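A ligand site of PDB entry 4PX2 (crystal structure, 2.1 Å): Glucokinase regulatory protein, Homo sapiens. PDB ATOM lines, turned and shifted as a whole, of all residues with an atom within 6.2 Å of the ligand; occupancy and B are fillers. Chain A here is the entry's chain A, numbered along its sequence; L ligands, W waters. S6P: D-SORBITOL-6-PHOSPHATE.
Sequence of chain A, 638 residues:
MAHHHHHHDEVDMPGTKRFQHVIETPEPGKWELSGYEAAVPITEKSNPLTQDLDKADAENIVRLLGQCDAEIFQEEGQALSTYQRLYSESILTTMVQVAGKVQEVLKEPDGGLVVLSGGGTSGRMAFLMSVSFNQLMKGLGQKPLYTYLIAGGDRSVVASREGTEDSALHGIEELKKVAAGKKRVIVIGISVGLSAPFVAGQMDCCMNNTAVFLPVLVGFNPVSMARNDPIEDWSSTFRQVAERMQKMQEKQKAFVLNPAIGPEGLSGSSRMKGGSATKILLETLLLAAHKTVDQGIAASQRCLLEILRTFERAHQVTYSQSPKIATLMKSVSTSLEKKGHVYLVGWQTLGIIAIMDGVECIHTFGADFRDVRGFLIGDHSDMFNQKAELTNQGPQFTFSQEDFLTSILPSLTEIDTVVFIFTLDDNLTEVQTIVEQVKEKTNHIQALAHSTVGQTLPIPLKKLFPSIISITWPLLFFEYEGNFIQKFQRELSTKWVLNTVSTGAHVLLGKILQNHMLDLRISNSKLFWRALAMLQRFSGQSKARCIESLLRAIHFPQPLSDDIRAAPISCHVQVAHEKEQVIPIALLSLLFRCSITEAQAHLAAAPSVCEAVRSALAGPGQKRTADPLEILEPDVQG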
ATOM      1  N   THR A  43     -16.919 -16.494  -1.388  1.00  0.00           N
ATOM      2  CA  THR A  43     -17.394 -16.960  -0.103  1.00  0.00           C
ATOM      3  C   THR A  43     -18.860 -16.654   0.097  1.00  0.00           C
ATOM      4  O   THR A  43     -19.423 -17.190   0.969  1.00  0.00           O
ATOM      5  CB  THR A  43     -16.605 -16.308   1.063  1.00  0.00           C
ATOM      6  OG1 THR A  43     -16.686 -14.875   1.016  1.00  0.00           O
ATOM      7  CG2 THR A  43     -15.170 -16.673   0.953  1.00  0.00           C
ATOM      8  N   GLY A 119     -12.441 -13.310  13.840  1.00  0.00           N
ATOM      9  CA  GLY A 119     -13.752 -13.190  14.466  1.00  0.00           C
ATOM     10  C   GLY A 119     -14.461 -14.488  14.276  1.00  0.00           C
ATOM     11  O   GLY A 119     -14.221 -15.228  13.291  1.00  0.00           O
ATOM     12  N   GLY A 120     -15.390 -14.773  15.162  1.00  0.00           N
ATOM     13  CA  GLY A 120     -16.331 -15.871  14.945  1.00  0.00           C
ATOM     14  C   GLY A 120     -15.509 -17.160  14.778  1.00  0.00           C
ATOM     15  O   GLY A 120     -14.535 -17.358  15.522  1.00  0.00           O
ATOM     16  N   THR A 121     -15.875 -18.001  13.791  1.00  0.00           N
ATOM     17  CA  THR A 121     -15.190 -19.282  13.591  1.00  0.00           C
ATOM     18  C   THR A 121     -13.750 -19.101  13.263  1.00  0.00           C
ATOM     19  O   THR A 121     -12.933 -19.939  13.642  1.00  0.00           O
ATOM     20  CB  THR A 121     -15.866 -20.131  12.536  1.00  0.00           C
ATOM     21  OG1 THR A 121     -17.229 -20.276  12.878  1.00  0.00           O
ATOM     22  CG2 THR A 121     -15.267 -21.494  12.463  1.00  0.00           C
ATOM     23  N   SER A 122     -13.360 -17.996  12.657  1.00  0.00           N
ATOM     24  CA  SER A 122     -11.934 -17.783  12.434  1.00  0.00           C
ATOM     25  C   SER A 122     -11.205 -17.640  13.719  1.00  0.00           C
ATOM     26  O   SER A 122     -10.044 -18.072  13.859  1.00  0.00           O
ATOM     27  CB  SER A 122     -11.701 -16.589  11.516  1.00  0.00           C
ATOM     28  OG  SER A 122     -12.332 -16.876  10.267  1.00  0.00           O
ATOM     29  N   ARG A 124     -12.248 -18.934  16.713  1.00  0.00           N
ATOM     30  CA  ARG A 124     -12.277 -20.263  17.206  1.00  0.00           C
ATOM     31  C   ARG A 124     -11.106 -21.122  16.642  1.00  0.00           C
ATOM     32  O   ARG A 124     -10.223 -21.574  17.415  1.00  0.00           O
ATOM     33  CB  ARG A 124     -13.621 -20.875  16.864  1.00  0.00           C
ATOM     34  CG  ARG A 124     -14.786 -20.318  17.690  1.00  0.00           C
ATOM     35  CD  ARG A 124     -16.043 -21.152  17.460  1.00  0.00           C
ATOM     36  NE  ARG A 124     -17.165 -20.343  16.957  1.00  0.00           N
ATOM     37  CZ  ARG A 124     -17.862 -19.477  17.708  1.00  0.00           C
ATOM     38  NH1 ARG A 124     -17.559 -19.320  18.995  1.00  0.00           N
ATOM     39  NH2 ARG A 124     -18.842 -18.787  17.201  1.00  0.00           N
ATOM     40  N   GLU A 162     -21.851 -12.697  17.280  1.00  0.00           N
ATOM     41  CA  GLU A 162     -21.613 -12.300  15.858  1.00  0.00           C
ATOM     42  C   GLU A 162     -21.399 -10.785  15.686  1.00  0.00           C
ATOM     43  O   GLU A 162     -20.746 -10.365  14.759  1.00  0.00           O
ATOM     44  CB  GLU A 162     -22.810 -12.781  15.036  1.00  0.00           C
ATOM     45  CG  GLU A 162     -22.803 -14.298  14.789  1.00  0.00           C
ATOM     46  CD  GLU A 162     -21.668 -14.683  13.829  1.00  0.00           C
ATOM     47  OE1 GLU A 162     -21.954 -14.842  12.608  1.00  0.00           O
ATOM     48  OE2 GLU A 162     -20.498 -14.729  14.282  1.00  0.00           O
ATOM     49  N   GLU A 165     -17.293  -8.638  15.644  1.00  0.00           N
ATOM     50  CA  GLU A 165     -16.280  -8.504  14.545  1.00  0.00           C
ATOM     51  C   GLU A 165     -16.203  -7.149  13.847  1.00  0.00           C
ATOM     52  O   GLU A 165     -15.279  -6.925  13.026  1.00  0.00           O
ATOM     53  CB  GLU A 165     -16.488  -9.552  13.493  1.00  0.00           C
ATOM     54  CG  GLU A 165     -17.755  -9.458  12.693  1.00  0.00           C
ATOM     55  CD  GLU A 165     -17.746 -10.422  11.533  1.00  0.00           C
ATOM     56  OE1 GLU A 165     -17.987 -11.617  11.768  1.00  0.00           O
ATOM     57  OE2 GLU A 165     -17.512  -9.977  10.390  1.00  0.00           O
ATOM     58  N   ILE A 190      -6.985 -13.847  10.286  1.00  0.00           N
ATOM     59  CA  ILE A 190      -7.752 -14.820   9.595  1.00  0.00           C
ATOM     60  C   ILE A 190      -9.166 -14.300   9.355  1.00  0.00           C
ATOM     61  O   ILE A 190      -9.941 -14.127  10.271  1.00  0.00           O
ATOM     62  CB  ILE A 190      -7.843 -16.092  10.449  1.00  0.00           C
ATOM     63  CG1 ILE A 190      -6.456 -16.691  10.795  1.00  0.00           C
ATOM     64  CG2 ILE A 190      -8.705 -17.070   9.712  1.00  0.00           C
ATOM     65  CD1 ILE A 190      -6.455 -17.814  11.859  1.00  0.00           C
ATOM     66  N   SER A 191      -9.507 -14.013   8.102  1.00  0.00           N
ATOM     67  CA  SER A 191     -10.875 -13.682   7.744  1.00  0.00           C
ATOM     68  C   SER A 191     -11.227 -14.343   6.421  1.00  0.00           C
ATOM     69  O   SER A 191     -10.772 -13.908   5.357  1.00  0.00           O
ATOM     70  CB  SER A 191     -11.102 -12.132   7.618  1.00  0.00           C
ATOM     71  OG  SER A 191     -12.494 -11.822   7.405  1.00  0.00           O
ATOM     72  N   VAL A 192     -12.106 -15.327   6.479  1.00  0.00           N
ATOM     73  CA  VAL A 192     -12.496 -16.056   5.320  1.00  0.00           C
ATOM     74  C   VAL A 192     -13.001 -15.228   4.114  1.00  0.00           C
ATOM     75  O   VAL A 192     -12.636 -15.457   2.948  1.00  0.00           O
ATOM     76  CB  VAL A 192     -13.570 -17.073   5.686  1.00  0.00           C
ATOM     77  CG1 VAL A 192     -14.056 -17.752   4.439  1.00  0.00           C
ATOM     78  CG2 VAL A 192     -12.963 -18.115   6.581  1.00  0.00           C
ATOM     79  N   GLY A 193     -13.881 -14.292   4.398  1.00  0.00           N
ATOM     80  CA  GLY A 193     -14.426 -13.410   3.391  1.00  0.00           C
ATOM     81  C   GLY A 193     -13.474 -12.292   3.068  1.00  0.00           C
ATOM     82  O   GLY A 193     -13.782 -11.501   2.180  1.00  0.00           O
ATOM     83  N   LEU A 194     -12.324 -12.197   3.767  1.00  0.00           N
ATOM     84  CA  LEU A 194     -11.473 -10.999   3.763  1.00  0.00           C
ATOM     85  C   LEU A 194     -12.465  -9.817   4.039  1.00  0.00           C
ATOM     86  O   LEU A 194     -12.687  -8.886   3.238  1.00  0.00           O
ATOM     87  CB  LEU A 194     -10.762 -10.813   2.409  1.00  0.00           C
ATOM     88  CG  LEU A 194      -9.715 -11.833   1.880  1.00  0.00           C
ATOM     89  CD1 LEU A 194      -9.007 -11.327   0.623  1.00  0.00           C
ATOM     90  CD2 LEU A 194      -8.641 -12.122   2.907  1.00  0.00           C
ATOM     91  N   SER A 195     -13.097  -9.921   5.192  1.00  0.00           N
ATOM     92  CA  SER A 195     -14.272  -9.207   5.517  1.00  0.00           C
ATOM     93  C   SER A 195     -14.216  -8.486   6.873  1.00  0.00           C
ATOM     94  O   SER A 195     -14.659  -7.318   6.950  1.00  0.00           O
ATOM     95  CB  SER A 195     -15.430 -10.183   5.519  1.00  0.00           C
ATOM     96  OG  SER A 195     -16.454  -9.715   6.334  1.00  0.00           O
ATOM     97  N   ALA A 196     -13.684  -9.137   7.932  1.00  0.00           N
ATOM     98  CA  ALA A 196     -13.897  -8.641   9.294  1.00  0.00           C
ATOM     99  C   ALA A 196     -13.107  -7.358   9.634  1.00  0.00           C
ATOM    100  O   ALA A 196     -11.894  -7.291   9.532  1.00  0.00           O
ATOM    101  CB  ALA A 196     -13.623  -9.744  10.325  1.00  0.00           C
ATOM    102  N   VAL A 199     -10.110  -7.698  11.814  1.00  0.00           N
ATOM    103  CA  VAL A 199      -8.852  -8.122  11.233  1.00  0.00           C
ATOM    104  C   VAL A 199      -8.273  -7.016  10.419  1.00  0.00           C
ATOM    105  O   VAL A 199      -7.086  -6.739  10.465  1.00  0.00           O
ATOM    106  CB  VAL A 199      -9.083  -9.407  10.351  1.00  0.00           C
ATOM    107  CG1 VAL A 199      -7.834  -9.808   9.579  1.00  0.00           C
ATOM    108  CG2 VAL A 199      -9.561 -10.569  11.224  1.00  0.00           C
ATOM    109  N   GLY A 268     -22.540 -18.820   2.227  1.00  0.00           N
ATOM    110  CA  GLY A 268     -22.030 -17.849   3.147  1.00  0.00           C
ATOM    111  C   GLY A 268     -21.700 -18.441   4.493  1.00  0.00           C
ATOM    112  O   GLY A 268     -21.179 -17.752   5.371  1.00  0.00           O
ATOM    113  N   SER A 269     -21.926 -19.738   4.648  1.00  0.00           N
ATOM    114  CA  SER A 269     -21.683 -20.297   5.942  1.00  0.00           C
ATOM    115  C   SER A 269     -20.175 -20.628   6.075  1.00  0.00           C
ATOM    116  O   SER A 269     -19.799 -21.782   5.985  1.00  0.00           O
ATOM    117  CB  SER A 269     -22.616 -21.521   6.219  1.00  0.00           C
ATOM    118  OG  SER A 269     -22.359 -22.023   7.503  1.00  0.00           O
ATOM    119  N   SER A 270     -19.342 -19.610   6.333  1.00  0.00           N
ATOM    120  CA  SER A 270     -17.894 -19.800   6.292  1.00  0.00           C
ATOM    121  C   SER A 270     -17.333 -20.609   7.503  1.00  0.00           C
ATOM    122  O   SER A 270     -16.105 -20.854   7.614  1.00  0.00           O
ATOM    123  CB  SER A 270     -17.226 -18.439   6.182  1.00  0.00           C
ATOM    124  OG  SER A 270     -17.444 -17.674   7.341  1.00  0.00           O
ATOM    125  N   ARG A 271     -18.197 -20.962   8.454  1.00  0.00           N
ATOM    126  CA  ARG A 271     -17.774 -21.865   9.529  1.00  0.00           C
ATOM    127  C   ARG A 271     -17.437 -23.299   9.027  1.00  0.00           C
ATOM    128  O   ARG A 271     -16.869 -24.074   9.777  1.00  0.00           O
ATOM    129  CB  ARG A 271     -18.870 -22.025  10.599  1.00  0.00           C
ATOM    130  CG  ARG A 271     -20.074 -22.869  10.142  1.00  0.00           C
ATOM    131  CD  ARG A 271     -21.276 -22.830  11.123  1.00  0.00           C
ATOM    132  NE  ARG A 271     -22.256 -23.945  10.873  1.00  0.00           N
ATOM    133  CZ  ARG A 271     -22.289 -25.091  11.575  1.00  0.00           C
ATOM    134  NH1 ARG A 271     -21.489 -25.264  12.638  1.00  0.00           N
ATOM    135  NH2 ARG A 271     -23.158 -26.051  11.299  1.00  0.00           N
ATOM    136  N   MET A 272     -17.904 -23.650   7.827  1.00  0.00           N
ATOM    137  CA  MET A 272     -17.715 -24.966   7.256  1.00  0.00           C
ATOM    138  C   MET A 272     -16.367 -25.061   6.527  1.00  0.00           C
ATOM    139  O   MET A 272     -15.331 -25.232   7.151  1.00  0.00           O
ATOM    140  CB  MET A 272     -18.887 -25.242   6.322  1.00  0.00           C
ATOM    141  CG  MET A 272     -20.175 -25.311   7.095  1.00  0.00           C
ATOM    142  SD  MET A 272     -21.635 -25.658   6.120  1.00  0.00           S
ATOM    143  CE  MET A 272     -21.671 -27.408   6.401  1.00  0.00           C
ATOM    144  N   GLU A 360     -22.651 -22.565  17.241  1.00  0.00           N
ATOM    145  CA  GLU A 360     -22.728 -21.949  15.910  1.00  0.00           C
ATOM    146  C   GLU A 360     -24.092 -22.148  15.333  1.00  0.00           C
ATOM    147  O   GLU A 360     -24.553 -21.327  14.517  1.00  0.00           O
ATOM    148  CB  GLU A 360     -21.632 -22.473  14.994  1.00  0.00           C
ATOM    149  CG  GLU A 360     -20.269 -22.044  15.512  1.00  0.00           C
ATOM    150  CD  GLU A 360     -19.098 -22.628  14.724  1.00  0.00           C
ATOM    151  OE1 GLU A 360     -19.360 -23.632  14.036  1.00  0.00           O
ATOM    152  OE2 GLU A 360     -17.949 -22.065  14.797  1.00  0.00           O
ATOM    153  N   HIS A 363     -26.674 -18.776  15.836  1.00  0.00           N
ATOM    154  CA  HIS A 363     -26.715 -17.751  14.806  1.00  0.00           C
ATOM    155  C   HIS A 363     -26.952 -18.408  13.439  1.00  0.00           C
ATOM    156  O   HIS A 363     -27.781 -17.935  12.681  1.00  0.00           O
ATOM    157  CB  HIS A 363     -25.499 -16.845  14.911  1.00  0.00           C
ATOM    158  CG  HIS A 363     -24.164 -17.556  14.775  1.00  0.00           C
ATOM    159  ND1 HIS A 363     -23.264 -17.634  15.803  1.00  0.00           N
ATOM    160  CD2 HIS A 363     -23.541 -18.105  13.697  1.00  0.00           C
ATOM    161  CE1 HIS A 363     -22.158 -18.221  15.388  1.00  0.00           C
ATOM    162  NE2 HIS A 363     -22.309 -18.528  14.116  1.00  0.00           N
ATOM    163  N   THR A 364     -26.365 -19.557  13.133  1.00  0.00           N
ATOM    164  CA  THR A 364     -26.531 -20.074  11.768  1.00  0.00           C
ATOM    165  C   THR A 364     -27.971 -20.444  11.484  1.00  0.00           C
ATOM    166  O   THR A 364     -28.482 -20.223  10.385  1.00  0.00           O
ATOM    167  CB  THR A 364     -25.620 -21.288  11.496  1.00  0.00           C
ATOM    168  OG1 THR A 364     -24.281 -20.987  11.841  1.00  0.00           O
ATOM    169  CG2 THR A 364     -25.612 -21.681  10.071  1.00  0.00           C
ATOM    170  N   ASN A 524     -24.460  -8.285  12.243  1.00  0.00           N
ATOM    171  CA  ASN A 524     -23.266  -7.538  11.871  1.00  0.00           C
ATOM    172  C   ASN A 524     -23.422  -6.995  10.491  1.00  0.00           C
ATOM    173  O   ASN A 524     -24.369  -7.332   9.771  1.00  0.00           O
ATOM    174  CB  ASN A 524     -21.960  -8.363  12.066  1.00  0.00           C
ATOM    175  CG  ASN A 524     -21.939  -9.681  11.293  1.00  0.00           C
ATOM    176  OD1 ASN A 524     -21.476 -10.744  11.797  1.00  0.00           O
ATOM    177  ND2 ASN A 524     -22.330  -9.632  10.041  1.00  0.00           N
ATOM    178  N   LYS A 526     -21.765  -7.592   7.714  1.00  0.00           N
ATOM    179  CA  LYS A 526     -21.745  -8.617   6.641  1.00  0.00           C
ATOM    180  C   LYS A 526     -23.093  -9.268   6.431  1.00  0.00           C
ATOM    181  O   LYS A 526     -23.567  -9.386   5.305  1.00  0.00           O
ATOM    182  CB  LYS A 526     -20.692  -9.696   6.994  1.00  0.00           C
ATOM    183  CG  LYS A 526     -20.565 -10.816   6.010  1.00  0.00           C
ATOM    184  CD  LYS A 526     -19.343 -11.750   6.297  1.00  0.00           C
ATOM    185  CE  LYS A 526     -19.498 -12.513   7.592  1.00  0.00           C
ATOM    186  NZ  LYS A 526     -18.147 -13.025   7.841  1.00  0.00           N
ATOM    187  N   ARG A 530     -25.620  -9.560   3.322  1.00  0.00           N
ATOM    188  CA  ARG A 530     -26.082 -10.853   2.849  1.00  0.00           C
ATOM    189  C   ARG A 530     -27.602 -10.797   2.742  1.00  0.00           C
ATOM    190  O   ARG A 530     -28.183 -11.254   1.733  1.00  0.00           O
ATOM    191  CB  ARG A 530     -25.594 -12.013   3.740  1.00  0.00           C
ATOM    192  CG  ARG A 530     -25.928 -13.401   3.205  1.00  0.00           C
ATOM    193  CD  ARG A 530     -25.240 -14.489   4.009  1.00  0.00           C
ATOM    194  NE  ARG A 530     -23.777 -14.269   4.121  1.00  0.00           N
ATOM    195  CZ  ARG A 530     -23.020 -14.704   5.119  1.00  0.00           C
ATOM    196  NH1 ARG A 530     -23.587 -15.356   6.097  1.00  0.00           N
ATOM    197  NH2 ARG A 530     -21.705 -14.433   5.197  1.00  0.00           N
HETATM  198  C1  S6P L   1     -19.808 -18.000   9.498  1.00  0.00           C
HETATM  199  C2  S6P L   1     -19.726 -17.806  10.990  1.00  0.00           C
HETATM  200  C3  S6P L   1     -19.250 -16.464  11.340  1.00  0.00           C
HETATM  201  C4  S6P L   1     -17.928 -16.200  10.656  1.00  0.00           C
HETATM  202  C5  S6P L   1     -17.525 -14.854  11.170  1.00  0.00           C
HETATM  203  C6  S6P L   1     -16.181 -14.499  10.625  1.00  0.00           C
HETATM  204  O1  S6P L   1     -20.463 -19.279   9.374  1.00  0.00           O
HETATM  205  O2  S6P L   1     -21.046 -18.000  11.536  1.00  0.00           O
HETATM  206  O3  S6P L   1     -19.053 -16.396  12.753  1.00  0.00           O
HETATM  207  O4  S6P L   1     -16.942 -17.149  11.064  1.00  0.00           O
HETATM  208  O5  S6P L   1     -18.553 -13.944  10.722  1.00  0.00           O
HETATM  209  O6  S6P L   1     -16.125 -14.623   9.191  1.00  0.00           O
HETATM  210  P   S6P L   1     -14.806 -14.206   8.422  1.00  0.00           P
HETATM  211  O1P S6P L   1     -15.140 -14.186   6.959  1.00  0.00           O
HETATM  212  O2P S6P L   1     -13.772 -15.372   8.728  1.00  0.00           O
HETATM  213  O3P S6P L   1     -14.117 -12.898   8.824  1.00  0.00           O
HETATM  214  O   HOH W   1     -15.408 -17.456   8.941  1.00  0.00           O
HETATM  215  O   HOH W   2     -16.485 -11.295   8.462  1.00  0.00           O
HETATM  216  O   HOH W   3     -17.179 -14.902   5.619  1.00  0.00           O
HETATM  217  O   HOH W   4     -18.435 -13.251  13.893  1.00  0.00           O
HETATM  218  O   HOH W   5     -21.005 -13.351  10.685  1.00  0.00           O
HETATM  219  O   HOH W   6     -12.366 -12.781  10.948  1.00  0.00           O
HETATM  220  O   HOH W   7     -19.302 -18.862  14.155  1.00  0.00           O
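The side-chain carboxylate of Glu 162 is in hydrogen-bond range of an oxygen (O3) of the ligand (2.7 Å). A ring nitrogen (NE2) of His 363 sits at hydrogen-bond distance from an oxygen (O2) of the ligand (2.9 Å). An oxygen (O1P) of the ligand is in salt-bridge range of the side-chain amino group (NZ) of Lys 526 (3.3 Å). The backbone NH of Arg 271 lies within hydrogen-bond range of an oxygen (O1) of the ligand (3.0 Å). An oxygen (O4) of the ligand is in hydrogen-bond range of the backbone NH (N) of Thr 121 (3.0 Å). The backbone NH (N) of Gly 193 lies within hydrogen-bond range of an oxygen (O1P) of the ligand (2.9 Å). OG of Ser 191 sits at hydrogen-bond distance from O3P of the ligand (2.4 Å). OG of Ser 122 sits at hydrogen-bond distance from O2P of the ligand (2.6 Å). The backbone NH (N) of Ser 270 sits at hydrogen-bond distance from an oxygen (O1) of the ligand, 3.3 Å away. An oxygen (O2P) of the ligand lies within hydrogen-bond range of the backbone NH (N) of Val 192, at 2.8 Å. OE1 of Glu 165 lies within hydrogen-bond range of O5 of the ligand (2.6 Å).
The backbone NH (N) of Ala 196 sits at hydrogen-bond distance from the side-chain hydroxyl (OG) of Ser 191 (3.0 Å). The side-chain carboxylate of Glu 360 sits at hydrogen-bond distance from the side-chain hydroxyl of Thr 121. The side-chain amide oxygen (OD1) of Asn 524 sits close to the backbone carbonyl oxygen (O) of Glu 162 (3.1 Å). The side-chain amide nitrogen (ND2) of Asn 524 lies close to the backbone NH (N) of Lys 526. OG of Ser 191 is in hydrogen-bond range of N of Ser 195, at 3.0 Å. The guanidinium group (NH1) of Arg 271 lies within salt-bridge range of the side-chain carboxylate (OE1) of Glu 360 (3.0 Å).
Gly 119 touches the ligand (O to C6, 3.4 Å). Gly 120 touches the ligand (CA to O3, 3.5 Å). CB of Ala 196 touches O3P of the ligand, at 3.5 Å. Ser 269 touches the ligand (C to O1, 3.6 Å). Within 4 Å of the ligand: Gly 119, Gly 120, Thr 121, Ser 122, Glu 162, Glu 165, Ser 191, Val 192, Gly 193, Ala 196, Ser 269, Ser 270, Arg 271, His 363 and Lys 526. The nearest printed residue that does not touch the ligand is Ser 195 (4.3 Å).
Water W5 lies within hydrogen-bond range of an oxygen (O5) of the ligand (2.5 Å), the side-chain carboxylate of Glu 162 (2.6 Å) and the side-chain amide oxygen of Asn 524 (2.9 Å). Water W3 lies within hydrogen-bond range of O1P of the ligand (2.5 Å), NZ of Lys 526 (3.1 Å) and OG of Ser 270 (3.3 Å). Water W1 lies within hydrogen-bond range of OG of Ser 270 (2.6 Å), O4 of the ligand (2.6 Å) and OG of Ser 122 (3.4 Å). Water W6 lies within hydrogen-bond range of O3P of the ligand (2.8 Å), O of Ile 190 (2.9 Å) and N of Gly 119 (2.9 Å). Water W2 lies within hydrogen-bond range of the side-chain amino group (NZ) of Lys 526, the side-chain carboxylate (OE2) of Glu 165, the side-chain hydroxyl (OG) of Ser 195 and an oxygen (O3P) of the ligand. Water W4 lies within hydrogen-bond range of the side-chain carboxylate (OE2) of Glu 162, the side-chain carboxylate (OE1) of Glu 165 and an oxygen (O5) of the ligand.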
